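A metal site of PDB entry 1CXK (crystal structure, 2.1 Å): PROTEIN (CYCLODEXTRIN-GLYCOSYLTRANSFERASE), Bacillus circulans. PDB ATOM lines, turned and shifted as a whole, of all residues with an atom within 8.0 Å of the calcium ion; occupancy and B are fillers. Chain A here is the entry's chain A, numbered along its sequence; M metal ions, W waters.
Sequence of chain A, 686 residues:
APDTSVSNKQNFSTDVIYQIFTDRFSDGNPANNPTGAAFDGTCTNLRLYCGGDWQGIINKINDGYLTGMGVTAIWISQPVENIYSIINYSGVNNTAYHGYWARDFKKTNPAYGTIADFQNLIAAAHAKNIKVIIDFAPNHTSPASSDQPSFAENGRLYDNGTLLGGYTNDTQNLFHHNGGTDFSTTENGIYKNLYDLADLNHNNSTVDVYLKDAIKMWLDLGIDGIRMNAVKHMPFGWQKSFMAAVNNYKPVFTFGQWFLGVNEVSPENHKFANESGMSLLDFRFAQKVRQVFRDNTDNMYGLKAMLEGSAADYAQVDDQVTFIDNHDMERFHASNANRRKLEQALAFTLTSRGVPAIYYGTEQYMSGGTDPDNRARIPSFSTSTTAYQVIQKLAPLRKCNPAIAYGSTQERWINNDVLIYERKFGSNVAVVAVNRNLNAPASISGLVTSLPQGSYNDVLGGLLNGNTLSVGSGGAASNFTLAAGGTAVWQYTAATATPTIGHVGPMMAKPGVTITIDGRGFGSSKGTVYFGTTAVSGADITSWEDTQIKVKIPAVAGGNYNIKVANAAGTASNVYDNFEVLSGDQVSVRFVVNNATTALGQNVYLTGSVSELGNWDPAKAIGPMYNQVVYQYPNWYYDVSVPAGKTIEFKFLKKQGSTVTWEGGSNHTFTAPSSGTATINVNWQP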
ATOM      1  N   THR A  22     -15.863  -5.374  14.258  1.00  0.00           N
ATOM      2  CA  THR A  22     -16.841  -4.311  14.376  1.00  0.00           C
ATOM      3  C   THR A  22     -17.645  -4.229  15.661  1.00  0.00           C
ATOM      4  O   THR A  22     -17.708  -3.181  16.292  1.00  0.00           O
ATOM      5  CB  THR A  22     -17.721  -4.208  13.127  1.00  0.00           C
ATOM      6  OG1 THR A  22     -16.898  -4.262  11.978  1.00  0.00           O
ATOM      7  CG2 THR A  22     -18.525  -2.908  13.147  1.00  0.00           C
ATOM      8  N   ASP A  23     -18.247  -5.342  16.054  1.00  0.00           N
ATOM      9  CA  ASP A  23     -19.064  -5.368  17.248  1.00  0.00           C
ATOM     10  C   ASP A  23     -18.319  -5.079  18.547  1.00  0.00           C
ATOM     11  O   ASP A  23     -18.920  -4.634  19.519  1.00  0.00           O
ATOM     12  CB  ASP A  23     -19.835  -6.691  17.382  1.00  0.00           C
ATOM     13  CG  ASP A  23     -20.851  -6.647  18.493  1.00  0.00           C
ATOM     14  OD1 ASP A  23     -21.795  -5.881  18.494  1.00  0.00           O
ATOM     15  OD2 ASP A  23     -20.586  -7.496  19.468  1.00  0.00           O
ATOM     16  N   SER A  26     -16.281  -0.155  18.782  1.00  0.00           N
ATOM     17  CA  SER A  26     -16.905   1.022  19.353  1.00  0.00           C
ATOM     18  C   SER A  26     -18.345   1.235  18.938  1.00  0.00           C
ATOM     19  O   SER A  26     -18.651   1.389  17.755  1.00  0.00           O
ATOM     20  CB  SER A  26     -16.063   2.245  19.058  1.00  0.00           C
ATOM     21  OG  SER A  26     -16.683   3.401  19.583  1.00  0.00           O
ATOM     22  N   ASP A  27     -19.233   1.267  19.917  1.00  0.00           N
ATOM     23  CA  ASP A  27     -20.641   1.480  19.665  1.00  0.00           C
ATOM     24  C   ASP A  27     -20.910   2.973  19.525  1.00  0.00           C
ATOM     25  O   ASP A  27     -21.131   3.654  20.519  1.00  0.00           O
ATOM     26  CB  ASP A  27     -21.514   0.869  20.767  1.00  0.00           C
ATOM     27  CG  ASP A  27     -22.968   1.197  20.649  1.00  0.00           C
ATOM     28  OD1 ASP A  27     -23.490   1.627  19.642  1.00  0.00           O
ATOM     29  OD2 ASP A  27     -23.624   0.930  21.754  1.00  0.00           O
ATOM     30  N   GLY A  28     -20.865   3.467  18.285  1.00  0.00           N
ATOM     31  CA  GLY A  28     -21.088   4.890  18.032  1.00  0.00           C
ATOM     32  C   GLY A  28     -22.555   5.245  17.813  1.00  0.00           C
ATOM     33  O   GLY A  28     -22.896   6.417  17.735  1.00  0.00           O
ATOM     34  N   ASN A  29     -23.411   4.234  17.713  1.00  0.00           N
ATOM     35  CA  ASN A  29     -24.836   4.437  17.513  1.00  0.00           C
ATOM     36  C   ASN A  29     -25.671   3.399  18.246  1.00  0.00           C
ATOM     37  O   ASN A  29     -26.063   2.366  17.704  1.00  0.00           O
ATOM     38  CB  ASN A  29     -25.239   4.511  16.027  1.00  0.00           C
ATOM     39  CG  ASN A  29     -26.727   4.800  15.846  1.00  0.00           C
ATOM     40  OD1 ASN A  29     -27.451   5.038  16.824  1.00  0.00           O
ATOM     41  ND2 ASN A  29     -27.174   4.795  14.594  1.00  0.00           N
ATOM     42  N   PRO A  30     -25.925   3.692  19.515  1.00  0.00           N
ATOM     43  CA  PRO A  30     -26.694   2.809  20.374  1.00  0.00           C
ATOM     44  C   PRO A  30     -28.080   2.509  19.840  1.00  0.00           C
ATOM     45  O   PRO A  30     -28.677   1.477  20.162  1.00  0.00           O
ATOM     46  CB  PRO A  30     -26.782   3.503  21.731  1.00  0.00           C
ATOM     47  CG  PRO A  30     -25.905   4.740  21.678  1.00  0.00           C
ATOM     48  CD  PRO A  30     -25.408   4.876  20.249  1.00  0.00           C
ATOM     49  N   ALA A  31     -28.595   3.416  19.004  1.00  0.00           N
ATOM     50  CA  ALA A  31     -29.918   3.269  18.429  1.00  0.00           C
ATOM     51  C   ALA A  31     -30.043   2.048  17.528  1.00  0.00           C
ATOM     52  O   ALA A  31     -31.126   1.526  17.327  1.00  0.00           O
ATOM     53  CB  ALA A  31     -30.319   4.531  17.682  1.00  0.00           C
ATOM     54  N   ASN A  32     -28.920   1.604  16.980  1.00  0.00           N
ATOM     55  CA  ASN A  32     -28.966   0.445  16.107  1.00  0.00           C
ATOM     56  C   ASN A  32     -28.652  -0.855  16.828  1.00  0.00           C
ATOM     57  O   ASN A  32     -28.626  -1.921  16.217  1.00  0.00           O
ATOM     58  CB  ASN A  32     -28.138   0.620  14.824  1.00  0.00           C
ATOM     59  CG  ASN A  32     -26.655   0.773  15.092  1.00  0.00           C
ATOM     60  OD1 ASN A  32     -26.140   0.231  16.074  1.00  0.00           O
ATOM     61  ND2 ASN A  32     -25.980   1.507  14.218  1.00  0.00           N
ATOM     62  N   ASN A  33     -28.399  -0.767  18.134  1.00  0.00           N
ATOM     63  CA  ASN A  33     -28.087  -1.959  18.893  1.00  0.00           C
ATOM     64  C   ASN A  33     -29.213  -2.967  18.867  1.00  0.00           C
ATOM     65  O   ASN A  33     -30.378  -2.595  18.938  1.00  0.00           O
ATOM     66  CB  ASN A  33     -27.789  -1.631  20.373  1.00  0.00           C
ATOM     67  CG  ASN A  33     -26.557  -0.781  20.565  1.00  0.00           C
ATOM     68  OD1 ASN A  33     -25.798  -0.533  19.607  1.00  0.00           O
ATOM     69  ND2 ASN A  33     -26.337  -0.344  21.798  1.00  0.00           N
ATOM     70  N   PRO A  34     -28.846  -4.246  18.801  1.00  0.00           N
ATOM     71  CA  PRO A  34     -29.858  -5.289  18.839  1.00  0.00           C
ATOM     72  C   PRO A  34     -30.444  -5.296  20.247  1.00  0.00           C
ATOM     73  O   PRO A  34     -29.838  -4.773  21.183  1.00  0.00           O
ATOM     74  CB  PRO A  34     -29.135  -6.598  18.507  1.00  0.00           C
ATOM     75  CG  PRO A  34     -27.821  -6.210  17.842  1.00  0.00           C
ATOM     76  CD  PRO A  34     -27.606  -4.734  18.145  1.00  0.00           C
ATOM     77  N   PHE A  39     -28.526  -9.199  23.102  1.00  0.00           N
ATOM     78  CA  PHE A  39     -27.591  -8.134  23.442  1.00  0.00           C
ATOM     79  C   PHE A  39     -27.118  -8.062  24.881  1.00  0.00           C
ATOM     80  O   PHE A  39     -27.851  -8.309  25.828  1.00  0.00           O
ATOM     81  CB  PHE A  39     -28.300  -6.816  23.071  1.00  0.00           C
ATOM     82  CG  PHE A  39     -27.469  -5.579  23.287  1.00  0.00           C
ATOM     83  CD1 PHE A  39     -26.519  -5.185  22.335  1.00  0.00           C
ATOM     84  CD2 PHE A  39     -27.650  -4.773  24.417  1.00  0.00           C
ATOM     85  CE1 PHE A  39     -25.761  -4.033  22.520  1.00  0.00           C
ATOM     86  CE2 PHE A  39     -26.901  -3.625  24.616  1.00  0.00           C
ATOM     87  CZ  PHE A  39     -25.954  -3.258  23.653  1.00  0.00           C
ATOM     88  N   TYR A  49     -24.314  -9.661  20.927  1.00  0.00           N
ATOM     89  CA  TYR A  49     -23.883  -8.393  20.360  1.00  0.00           C
ATOM     90  C   TYR A  49     -23.536  -7.427  21.473  1.00  0.00           C
ATOM     91  O   TYR A  49     -24.279  -7.332  22.452  1.00  0.00           O
ATOM     92  CB  TYR A  49     -24.967  -7.722  19.477  1.00  0.00           C
ATOM     93  CG  TYR A  49     -25.063  -8.183  18.047  1.00  0.00           C
ATOM     94  CD1 TYR A  49     -25.920  -9.231  17.693  1.00  0.00           C
ATOM     95  CD2 TYR A  49     -24.356  -7.551  17.028  1.00  0.00           C
ATOM     96  CE1 TYR A  49     -26.050  -9.652  16.368  1.00  0.00           C
ATOM     97  CE2 TYR A  49     -24.461  -7.955  15.689  1.00  0.00           C
ATOM     98  CZ  TYR A  49     -25.320  -9.014  15.366  1.00  0.00           C
ATOM     99  OH  TYR A  49     -25.445  -9.424  14.068  1.00  0.00           O
ATOM    100  N   CYS A  50     -22.430  -6.701  21.330  1.00  0.00           N
ATOM    101  CA  CYS A  50     -22.030  -5.739  22.334  1.00  0.00           C
ATOM    102  C   CYS A  50     -22.383  -4.325  21.921  1.00  0.00           C
ATOM    103  O   CYS A  50     -22.427  -3.426  22.748  1.00  0.00           O
ATOM    104  CB  CYS A  50     -20.564  -5.876  22.760  1.00  0.00           C
ATOM    105  SG  CYS A  50     -20.188  -7.532  23.407  1.00  0.00           S
ATOM    106  N   GLY A  51     -22.636  -4.129  20.615  1.00  0.00           N
ATOM    107  CA  GLY A  51     -23.042  -2.825  20.092  1.00  0.00           C
ATOM    108  C   GLY A  51     -22.081  -2.098  19.148  1.00  0.00           C
ATOM    109  O   GLY A  51     -22.451  -1.075  18.585  1.00  0.00           O
ATOM    110  N   GLY A  52     -20.851  -2.604  18.986  1.00  0.00           N
ATOM    111  CA  GLY A  52     -19.887  -1.954  18.099  1.00  0.00           C
ATOM    112  C   GLY A  52     -20.450  -1.745  16.699  1.00  0.00           C
ATOM    113  O   GLY A  52     -21.103  -2.637  16.149  1.00  0.00           O
ATOM    114  N   ASP A  53     -20.209  -0.581  16.098  1.00  0.00           N
ATOM    115  CA  ASP A  53     -20.749  -0.320  14.771  1.00  0.00           C
ATOM    116  C   ASP A  53     -19.877   0.568  13.881  1.00  0.00           C
ATOM    117  O   ASP A  53     -18.806   1.018  14.268  1.00  0.00           O
ATOM    118  CB  ASP A  53     -22.159   0.296  14.897  1.00  0.00           C
ATOM    119  CG  ASP A  53     -22.163   1.540  15.748  1.00  0.00           C
ATOM    120  OD1 ASP A  53     -21.231   2.345  15.778  1.00  0.00           O
ATOM    121  OD2 ASP A  53     -23.256   1.672  16.472  1.00  0.00           O
ATOM    122  N   TRP A  54     -20.361   0.815  12.666  1.00  0.00           N
ATOM    123  CA  TRP A  54     -19.659   1.634  11.700  1.00  0.00           C
ATOM    124  C   TRP A  54     -19.503   3.077  12.168  1.00  0.00           C
ATOM    125  O   TRP A  54     -18.459   3.703  11.947  1.00  0.00           O
ATOM    126  CB  TRP A  54     -20.286   1.554  10.279  1.00  0.00           C
ATOM    127  CG  TRP A  54     -20.197   0.179   9.687  1.00  0.00           C
ATOM    128  CD1 TRP A  54     -19.269  -0.755   9.995  1.00  0.00           C
ATOM    129  CD2 TRP A  54     -21.068  -0.408   8.721  1.00  0.00           C
ATOM    130  NE1 TRP A  54     -19.498  -1.900   9.270  1.00  0.00           N
ATOM    131  CE2 TRP A  54     -20.603  -1.726   8.487  1.00  0.00           C
ATOM    132  CE3 TRP A  54     -22.206   0.030   8.038  1.00  0.00           C
ATOM    133  CZ2 TRP A  54     -21.232  -2.582   7.586  1.00  0.00           C
ATOM    134  CZ3 TRP A  54     -22.816  -0.816   7.145  1.00  0.00           C
ATOM    135  CH2 TRP A  54     -22.343  -2.113   6.930  1.00  0.00           C
ATOM    136  N   GLN A  55     -20.525   3.621  12.813  1.00  0.00           N
ATOM    137  CA  GLN A  55     -20.415   4.982  13.311  1.00  0.00           C
ATOM    138  C   GLN A  55     -19.266   5.065  14.301  1.00  0.00           C
ATOM    139  O   GLN A  55     -18.534   6.049  14.360  1.00  0.00           O
ATOM    140  CB  GLN A  55     -21.725   5.502  13.930  1.00  0.00           C
ATOM    141  CG  GLN A  55     -21.611   6.920  14.512  1.00  0.00           C
ATOM    142  CD  GLN A  55     -21.375   7.987  13.463  1.00  0.00           C
ATOM    143  OE1 GLN A  55     -22.133   8.082  12.478  1.00  0.00           O
ATOM    144  NE2 GLN A  55     -20.346   8.793  13.665  1.00  0.00           N
ATOM    145  N   GLY A  56     -19.117   3.996  15.082  1.00  0.00           N
ATOM    146  CA  GLY A  56     -18.054   3.920  16.060  1.00  0.00           C
ATOM    147  C   GLY A  56     -16.704   4.012  15.374  1.00  0.00           C
ATOM    148  O   GLY A  56     -15.814   4.741  15.803  1.00  0.00           O
ATOM    149  N   PRO A 110     -27.915  -4.411   9.785  1.00  0.00           N
ATOM    150  CA  PRO A 110     -28.424  -3.240  10.481  1.00  0.00           C
ATOM    151  C   PRO A 110     -27.717  -2.908  11.782  1.00  0.00           C
ATOM    152  O   PRO A 110     -27.671  -1.749  12.191  1.00  0.00           O
ATOM    153  CB  PRO A 110     -29.920  -3.466  10.731  1.00  0.00           C
ATOM    154  CG  PRO A 110     -30.215  -4.916  10.370  1.00  0.00           C
ATOM    155  CD  PRO A 110     -28.948  -5.493   9.755  1.00  0.00           C
ATOM    156  N   ALA A 111     -27.178  -3.921  12.452  1.00  0.00           N
ATOM    157  CA  ALA A 111     -26.474  -3.663  13.708  1.00  0.00           C
ATOM    158  C   ALA A 111     -25.246  -2.808  13.464  1.00  0.00           C
ATOM    159  O   ALA A 111     -24.894  -1.946  14.277  1.00  0.00           O
ATOM    160  CB  ALA A 111     -26.156  -4.952  14.456  1.00  0.00           C
ATOM    161  N   TYR A 112     -24.598  -3.042  12.309  1.00  0.00           N
ATOM    162  CA  TYR A 112     -23.413  -2.293  11.904  1.00  0.00           C
ATOM    163  C   TYR A 112     -23.824  -0.939  11.335  1.00  0.00           C
ATOM    164  O   TYR A 112     -23.174   0.080  11.566  1.00  0.00           O
ATOM    165  CB  TYR A 112     -22.511  -3.045  10.896  1.00  0.00           C
ATOM    166  CG  TYR A 112     -21.979  -4.401  11.351  1.00  0.00           C
ATOM    167  CD1 TYR A 112     -21.939  -4.779  12.690  1.00  0.00           C
ATOM    168  CD2 TYR A 112     -21.495  -5.299  10.400  1.00  0.00           C
ATOM    169  CE1 TYR A 112     -21.438  -6.028  13.079  1.00  0.00           C
ATOM    170  CE2 TYR A 112     -20.990  -6.540  10.766  1.00  0.00           C
ATOM    171  CZ  TYR A 112     -20.960  -6.905  12.116  1.00  0.00           C
ATOM    172  OH  TYR A 112     -20.475  -8.138  12.471  1.00  0.00           O
ATOM    173  N   GLY A 113     -24.924  -0.935  10.590  1.00  0.00           N
ATOM    174  CA  GLY A 113     -25.416   0.313  10.007  1.00  0.00           C
ATOM    175  C   GLY A 113     -26.130   0.108   8.697  1.00  0.00           C
ATOM    176  O   GLY A 113     -26.315  -1.017   8.235  1.00  0.00           O
HETATM  177 CA    CA M   1     -24.558   0.264  17.941  1.00  0.00          CA
HETATM  178  O   HOH W   1     -24.836  -1.942  16.985  1.00  0.00           O
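The nearest printed residue that does not touch the calcium ion is Pro 30 (4.01 Å).
The side-chain amide oxygen (OD1) of Asn 33 is bound to the calcium ion, at 2.2 Å.
OD2 of Asp 53 is bound to the calcium ion (2.4 Å).
The calcium ion is bound by water W1 (2.4 Å).
The calcium ion is bound by OD1 of Asp 27 (2.4 Å).
The side-chain amide oxygen (OD1) of Asn 32 is bound to the calcium ion, at 2.4 Å.
The backbone carbonyl oxygen (O) of Gly 51 binds the calcium ion, at 2.6 Å.
The backbone carbonyl oxygen (O) of Asn 29 is bound to the calcium ion, 2.6 Å away.
The backbone carbonyl oxygen (O) of Pro 30 sits close to the side-chain amide nitrogen (ND2) of Asn 33.
The backbone NH of Gly 28 is in hydrogen-bond range of the side-chain carboxylate of Asp 53 (2.8 Å).
The backbone carbonyl oxygen (O) of Ser 26 lies within hydrogen-bond range of the backbone NH (N) of Asp 53 (3.0 Å).
The side-chain carboxylate (OD1) of Asp 53 lies close to the backbone NH (N) of Gln 55, at 3.3 Å.
The side-chain carboxylate (OD1) of Asp 53 is in hydrogen-bond range of the backbone NH (N) of Gly 56, 2.8 Å away.
The side-chain amide oxygen (OD1) of Asn 32 sits close to the backbone carbonyl oxygen (O) of Ala 111 (3.1 Å).
The backbone NH of Gly 51 lies within hydrogen-bond range of the side-chain carboxylate of Asp 23, at 2.9 Å.
The side-chain amide oxygen (OD1) of Asn 29 is in hydrogen-bond range of the backbone NH (N) of Ala 31 (2.9 Å).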
